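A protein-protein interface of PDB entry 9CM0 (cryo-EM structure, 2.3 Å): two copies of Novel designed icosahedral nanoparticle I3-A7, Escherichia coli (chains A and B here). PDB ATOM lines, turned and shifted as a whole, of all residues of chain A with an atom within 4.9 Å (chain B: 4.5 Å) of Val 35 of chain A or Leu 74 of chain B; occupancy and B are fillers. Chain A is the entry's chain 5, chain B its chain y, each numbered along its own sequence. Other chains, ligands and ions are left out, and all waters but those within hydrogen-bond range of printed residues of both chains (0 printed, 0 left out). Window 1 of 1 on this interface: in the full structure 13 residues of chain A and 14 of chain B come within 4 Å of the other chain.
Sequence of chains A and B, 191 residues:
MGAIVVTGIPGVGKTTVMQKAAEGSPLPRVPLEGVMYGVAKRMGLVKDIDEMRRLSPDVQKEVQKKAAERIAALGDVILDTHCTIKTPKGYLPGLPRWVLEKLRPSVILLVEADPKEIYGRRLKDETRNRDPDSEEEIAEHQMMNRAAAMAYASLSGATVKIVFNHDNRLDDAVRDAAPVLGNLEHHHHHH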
ATOM      1  N   VAL A  30      -2.737 -21.682  10.151  1.00  0.00           N
ATOM      2  CA  VAL A  30      -2.799 -22.899   9.327  1.00  0.00           C
ATOM      3  C   VAL A  30      -2.773 -24.169  10.179  1.00  0.00           C
ATOM      4  O   VAL A  30      -1.764 -24.434  10.819  1.00  0.00           O
ATOM      5  CB  VAL A  30      -1.636 -22.879   8.319  1.00  0.00           C
ATOM      6  CG1 VAL A  30      -1.636 -24.117   7.432  1.00  0.00           C
ATOM      7  CG2 VAL A  30      -1.715 -21.670   7.381  1.00  0.00           C
ATOM      8  N   PRO A  31      -3.824 -25.004  10.191  1.00  0.00           N
ATOM      9  CA  PRO A  31      -3.744 -26.352  10.736  1.00  0.00           C
ATOM     10  C   PRO A  31      -3.120 -27.312   9.710  1.00  0.00           C
ATOM     11  O   PRO A  31      -3.606 -27.425   8.582  1.00  0.00           O
ATOM     12  CB  PRO A  31      -5.187 -26.715  11.068  1.00  0.00           C
ATOM     13  CG  PRO A  31      -5.997 -25.964  10.015  1.00  0.00           C
ATOM     14  CD  PRO A  31      -5.170 -24.710   9.742  1.00  0.00           C
ATOM     15  N   LEU A  32      -2.054 -28.026  10.076  1.00  0.00           N
ATOM     16  CA  LEU A  32      -1.333 -28.881   9.128  1.00  0.00           C
ATOM     17  C   LEU A  32      -2.176 -30.052   8.606  1.00  0.00           C
ATOM     18  O   LEU A  32      -2.115 -30.398   7.427  1.00  0.00           O
ATOM     19  CB  LEU A  32      -0.052 -29.400   9.788  1.00  0.00           C
ATOM     20  CG  LEU A  32       0.804 -30.303   8.882  1.00  0.00           C
ATOM     21  CD1 LEU A  32       1.217 -29.637   7.571  1.00  0.00           C
ATOM     22  CD2 LEU A  32       2.082 -30.679   9.629  1.00  0.00           C
ATOM     23  N   GLU A  33      -2.996 -30.654   9.462  1.00  0.00           N
ATOM     24  CA  GLU A  33      -3.862 -31.773   9.075  1.00  0.00           C
ATOM     25  C   GLU A  33      -4.908 -31.313   8.054  1.00  0.00           C
ATOM     26  O   GLU A  33      -5.190 -31.994   7.068  1.00  0.00           O
ATOM     27  CB  GLU A  33      -4.572 -32.367  10.305  1.00  0.00           C
ATOM     28  CG  GLU A  33      -3.647 -32.740  11.480  1.00  0.00           C
ATOM     29  CD  GLU A  33      -3.181 -31.556  12.350  1.00  0.00           C
ATOM     30  OE1 GLU A  33      -3.719 -30.438  12.202  1.00  0.00           O
ATOM     31  OE2 GLU A  33      -2.256 -31.751  13.172  1.00  0.00           O
ATOM     32  N   GLY A  34      -5.432 -30.102   8.256  1.00  0.00           N
ATOM     33  CA  GLY A  34      -6.337 -29.438   7.333  1.00  0.00           C
ATOM     34  C   GLY A  34      -5.707 -29.216   5.964  1.00  0.00           C
ATOM     35  O   GLY A  34      -6.306 -29.563   4.947  1.00  0.00           O
ATOM     36  N   VAL A  35      -4.471 -28.711   5.912  1.00  0.00           N
ATOM     37  CA  VAL A  35      -3.755 -28.569   4.636  1.00  0.00           C
ATOM     38  C   VAL A  35      -3.507 -29.919   3.982  1.00  0.00           C
ATOM     39  O   VAL A  35      -3.735 -30.060   2.785  1.00  0.00           O
ATOM     40  CB  VAL A  35      -2.426 -27.818   4.778  1.00  0.00           C
ATOM     41  CG1 VAL A  35      -1.680 -27.725   3.441  1.00  0.00           C
ATOM     42  CG2 VAL A  35      -2.688 -26.395   5.256  1.00  0.00           C
ATOM     43  N   MET A  36      -3.097 -30.938   4.737  1.00  0.00           N
ATOM     44  CA  MET A  36      -2.895 -32.273   4.175  1.00  0.00           C
ATOM     45  C   MET A  36      -4.178 -32.819   3.547  1.00  0.00           C
ATOM     46  O   MET A  36      -4.131 -33.349   2.440  1.00  0.00           O
ATOM     47  CB  MET A  36      -2.403 -33.239   5.248  1.00  0.00           C
ATOM     48  CG  MET A  36      -0.927 -33.019   5.578  1.00  0.00           C
ATOM     49  SD  MET A  36      -0.328 -34.026   6.956  1.00  0.00           S
ATOM     50  CE  MET A  36      -0.709 -35.694   6.368  1.00  0.00           C
ATOM     51  N   TYR A  37      -5.324 -32.649   4.210  1.00  0.00           N
ATOM     52  CA  TYR A  37      -6.617 -33.020   3.644  1.00  0.00           C
ATOM     53  C   TYR A  37      -6.898 -32.245   2.360  1.00  0.00           C
ATOM     54  O   TYR A  37      -7.189 -32.857   1.338  1.00  0.00           O
ATOM     55  CB  TYR A  37      -7.715 -32.825   4.693  1.00  0.00           C
ATOM     56  CG  TYR A  37      -9.136 -32.965   4.179  1.00  0.00           C
ATOM     57  CD1 TYR A  37      -9.556 -34.151   3.546  1.00  0.00           C
ATOM     58  CD2 TYR A  37     -10.043 -31.906   4.351  1.00  0.00           C
ATOM     59  CE1 TYR A  37     -10.876 -34.277   3.078  1.00  0.00           C
ATOM     60  CE2 TYR A  37     -11.368 -32.032   3.895  1.00  0.00           C
ATOM     61  CZ  TYR A  37     -11.787 -33.214   3.255  1.00  0.00           C
ATOM     62  OH  TYR A  37     -13.065 -33.293   2.800  1.00  0.00           O
ATOM     63  N   GLY A  38      -6.724 -30.922   2.370  1.00  0.00           N
ATOM     64  CA  GLY A  38      -6.874 -30.094   1.175  1.00  0.00           C
ATOM     65  C   GLY A  38      -5.982 -30.551   0.016  1.00  0.00           C
ATOM     66  O   GLY A  38      -6.458 -30.716  -1.104  1.00  0.00           O
ATOM     67  N   VAL A  39      -4.703 -30.825   0.269  1.00  0.00           N
ATOM     68  CA  VAL A  39      -3.771 -31.301  -0.760  1.00  0.00           C
ATOM     69  C   VAL A  39      -4.187 -32.670  -1.292  1.00  0.00           C
ATOM     70  O   VAL A  39      -4.310 -32.835  -2.500  1.00  0.00           O
ATOM     71  CB  VAL A  39      -2.329 -31.303  -0.216  1.00  0.00           C
ATOM     72  CG1 VAL A  39      -1.331 -31.995  -1.149  1.00  0.00           C
ATOM     73  CG2 VAL A  39      -1.847 -29.860  -0.034  1.00  0.00           C
ATOM     74  N   ALA A  40      -4.491 -33.635  -0.423  1.00  0.00           N
ATOM     75  CA  ALA A  40      -4.928 -34.960  -0.853  1.00  0.00           C
ATOM     76  C   ALA A  40      -6.253 -34.906  -1.634  1.00  0.00           C
ATOM     77  O   ALA A  40      -6.389 -35.552  -2.673  1.00  0.00           O
ATOM     78  CB  ALA A  40      -5.047 -35.846   0.388  1.00  0.00           C
ATOM     79  N   ALA A  67       2.351 -30.914   1.123  1.00  0.00           N
ATOM     80  CA  ALA A  67       1.747 -29.948   2.034  1.00  0.00           C
ATOM     81  C   ALA A  67       2.811 -29.023   2.642  1.00  0.00           C
ATOM     82  O   ALA A  67       2.651 -27.804   2.638  1.00  0.00           O
ATOM     83  CB  ALA A  67       0.972 -30.706   3.113  1.00  0.00           C
ATOM     84  N   ARG A  70       4.146 -26.500  -0.018  1.00  0.00           N
ATOM     85  CA  ARG A  70       3.158 -25.437  -0.243  1.00  0.00           C
ATOM     86  C   ARG A  70       3.071 -24.472   0.931  1.00  0.00           C
ATOM     87  O   ARG A  70       2.992 -23.268   0.710  1.00  0.00           O
ATOM     88  CB  ARG A  70       1.803 -26.069  -0.564  1.00  0.00           C
ATOM     89  CG  ARG A  70       1.863 -26.765  -1.930  1.00  0.00           C
ATOM     90  CD  ARG A  70       0.586 -27.552  -2.205  1.00  0.00           C
ATOM     91  NE  ARG A  70       0.701 -28.285  -3.474  1.00  0.00           N
ATOM     92  CZ  ARG A  70      -0.272 -28.669  -4.277  1.00  0.00           C
ATOM     93  NH1 ARG A  70      -0.004 -29.422  -5.300  1.00  0.00           N
ATOM     94  NH2 ARG A  70      -1.514 -28.323  -4.103  1.00  0.00           N
ATOM     95  N   ILE A  71       3.163 -24.954   2.168  1.00  0.00           N
ATOM     96  CA  ILE A  71       3.231 -24.070   3.340  1.00  0.00           C
ATOM     97  C   ILE A  71       4.552 -23.290   3.362  1.00  0.00           C
ATOM     98  O   ILE A  71       4.563 -22.128   3.754  1.00  0.00           O
ATOM     99  CB  ILE A  71       3.008 -24.869   4.633  1.00  0.00           C
ATOM    100  CG1 ILE A  71       1.579 -25.447   4.690  1.00  0.00           C
ATOM    101  CG2 ILE A  71       3.215 -23.985   5.871  1.00  0.00           C
ATOM    102  CD1 ILE A  71       1.486 -26.637   5.649  1.00  0.00           C
ATOM    103  N   LEU A  74       4.087 -20.370   0.798  1.00  0.00           N
ATOM    104  CA  LEU A  74       3.276 -19.310   1.406  1.00  0.00           C
ATOM    105  C   LEU A  74       4.113 -18.340   2.257  1.00  0.00           C
ATOM    106  O   LEU A  74       3.709 -17.202   2.475  1.00  0.00           O
ATOM    107  CB  LEU A  74       2.182 -19.979   2.258  1.00  0.00           C
ATOM    108  CG  LEU A  74       1.101 -19.032   2.802  1.00  0.00           C
ATOM    109  CD1 LEU A  74       0.188 -18.556   1.677  1.00  0.00           C
ATOM    110  CD2 LEU A  74       0.245 -19.750   3.841  1.00  0.00           C
ATOM    111  N   PRO B  28      -7.685 -23.600   6.552  1.00  0.00           N
ATOM    112  CA  PRO B  28      -6.778 -22.538   6.963  1.00  0.00           C
ATOM    113  C   PRO B  28      -7.434 -21.166   6.821  1.00  0.00           C
ATOM    114  O   PRO B  28      -8.340 -20.993   6.003  1.00  0.00           O
ATOM    115  CB  PRO B  28      -5.551 -22.671   6.059  1.00  0.00           C
ATOM    116  CG  PRO B  28      -6.092 -23.341   4.804  1.00  0.00           C
ATOM    117  CD  PRO B  28      -7.226 -24.216   5.322  1.00  0.00           C
ATOM    118  N   VAL B  30      -6.558 -16.897   6.184  1.00  0.00           N
ATOM    119  CA  VAL B  30      -5.503 -16.124   5.531  1.00  0.00           C
ATOM    120  C   VAL B  30      -5.936 -14.671   5.347  1.00  0.00           C
ATOM    121  O   VAL B  30      -6.931 -14.437   4.669  1.00  0.00           O
ATOM    122  CB  VAL B  30      -5.176 -16.773   4.174  1.00  0.00           C
ATOM    123  CG1 VAL B  30      -4.139 -15.964   3.409  1.00  0.00           C
ATOM    124  CG2 VAL B  30      -4.613 -18.188   4.325  1.00  0.00           C
ATOM    125  N   ARG B  70      -0.015 -18.679  -4.984  1.00  0.00           N
ATOM    126  CA  ARG B  70       0.390 -19.446  -3.799  1.00  0.00           C
ATOM    127  C   ARG B  70      -0.799 -19.812  -2.919  1.00  0.00           C
ATOM    128  O   ARG B  70      -0.851 -20.933  -2.420  1.00  0.00           O
ATOM    129  CB  ARG B  70       1.471 -18.671  -3.044  1.00  0.00           C
ATOM    130  CG  ARG B  70       2.759 -18.632  -3.874  1.00  0.00           C
ATOM    131  CD  ARG B  70       3.783 -17.695  -3.245  1.00  0.00           C
ATOM    132  NE  ARG B  70       4.981 -17.596  -4.094  1.00  0.00           N
ATOM    133  CZ  ARG B  70       6.223 -17.377  -3.708  1.00  0.00           C
ATOM    134  NH1 ARG B  70       7.148 -17.178  -4.596  1.00  0.00           N
ATOM    135  NH2 ARG B  70       6.581 -17.356  -2.457  1.00  0.00           N
ATOM    136  N   ILE B  71      -1.797 -18.941  -2.783  1.00  0.00           N
ATOM    137  CA  ILE B  71      -3.036 -19.287  -2.071  1.00  0.00           C
ATOM    138  C   ILE B  71      -3.865 -20.304  -2.871  1.00  0.00           C
ATOM    139  O   ILE B  71      -4.484 -21.186  -2.287  1.00  0.00           O
ATOM    140  CB  ILE B  71      -3.841 -18.020  -1.733  1.00  0.00           C
ATOM    141  CG1 ILE B  71      -3.068 -17.139  -0.733  1.00  0.00           C
ATOM    142  CG2 ILE B  71      -5.205 -18.377  -1.122  1.00  0.00           C
ATOM    143  CD1 ILE B  71      -3.549 -15.685  -0.750  1.00  0.00           C
ATOM    144  N   ALA B  72      -3.840 -20.260  -4.199  1.00  0.00           N
ATOM    145  CA  ALA B  72      -4.499 -21.276  -5.014  1.00  0.00           C
ATOM    146  C   ALA B  72      -3.846 -22.658  -4.838  1.00  0.00           C
ATOM    147  O   ALA B  72      -4.545 -23.665  -4.715  1.00  0.00           O
ATOM    148  CB  ALA B  72      -4.485 -20.823  -6.477  1.00  0.00           C
ATOM    149  N   ALA B  73      -2.513 -22.724  -4.766  1.00  0.00           N
ATOM    150  CA  ALA B  73      -1.799 -23.971  -4.517  1.00  0.00           C
ATOM    151  C   ALA B  73      -2.118 -24.567  -3.134  1.00  0.00           C
ATOM    152  O   ALA B  73      -2.270 -25.781  -3.010  1.00  0.00           O
ATOM    153  CB  ALA B  73      -0.300 -23.713  -4.685  1.00  0.00           C
ATOM    154  N   LEU B  74      -2.268 -23.730  -2.102  1.00  0.00           N
ATOM    155  CA  LEU B  74      -2.707 -24.156  -0.765  1.00  0.00           C
ATOM    156  C   LEU B  74      -4.087 -24.829  -0.786  1.00  0.00           C
ATOM    157  O   LEU B  74      -4.358 -25.714   0.022  1.00  0.00           O
ATOM    158  CB  LEU B  74      -2.711 -22.924   0.157  1.00  0.00           C
ATOM    159  CG  LEU B  74      -3.063 -23.208   1.625  1.00  0.00           C
ATOM    160  CD1 LEU B  74      -1.943 -23.995   2.297  1.00  0.00           C
ATOM    161  CD2 LEU B  74      -3.251 -21.903   2.389  1.00  0.00           C
ATOM    162  N   GLY B  75      -4.944 -24.445  -1.728  1.00  0.00           N
ATOM    163  CA  GLY B  75      -6.256 -25.043  -1.938  1.00  0.00           C
ATOM    164  C   GLY B  75      -7.386 -24.366  -1.165  1.00  0.00           C
ATOM    165  O   GLY B  75      -7.433 -23.146  -1.046  1.00  0.00           O
ATOM    166  N   ASP B  76      -8.342 -25.155  -0.683  1.00  0.00           N
ATOM    167  CA  ASP B  76      -9.557 -24.640  -0.042  1.00  0.00           C
ATOM    168  C   ASP B  76      -9.201 -23.870   1.242  1.00  0.00           C
ATOM    169  O   ASP B  76      -8.470 -24.379   2.086  1.00  0.00           O
ATOM    170  CB  ASP B  76     -10.561 -25.769   0.258  1.00  0.00           C
ATOM    171  CG  ASP B  76     -10.904 -26.726  -0.902  1.00  0.00           C
ATOM    172  OD1 ASP B  76     -10.338 -26.614  -2.015  1.00  0.00           O
ATOM    173  OD2 ASP B  76     -11.750 -27.624  -0.677  1.00  0.00           O
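Of the printed residues of chain B, Pro 31 of chain A touches Pro 28 (3.9 Å). Val 35 of chain A touches one residue of chain B. Printed residues of chain B within 4 Å of Arg 70 of chain A: Ala 73 (2.9 Å). Of the printed residues of chain A, Pro 28 of chain B touches Pro 31 (3.9 Å). Printed residues of chain A within 4 Å of Ala 73 of chain B: Arg 70 (2.9 Å). Of chain A, only Val 35 comes within 4 Å of Leu 74 of chain B. The nearest printed residue of chain B that does not touch Val 35 of chain A is Pro 28 of chain B (4.6 Å). The nearest printed residue of chain A that does not touch Ala 73 of chain B is Val 39 of chain A (5.1 Å).
Of the 15 printed residues of chain A, 3 touch a printed residue of chain B.
4 positions are printed for both chains.
The guanidinium group of Arg 70 of chain A sits at hydrogen-bond distance from the backbone carbonyl oxygen of Ala 73 of chain B (2.9 Å).
Among the printed residues, merely in contact across the chains: Pro 31 of chain A with Pro 28 of chain B and Val 35 of chain A with Leu 74 of chain B.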
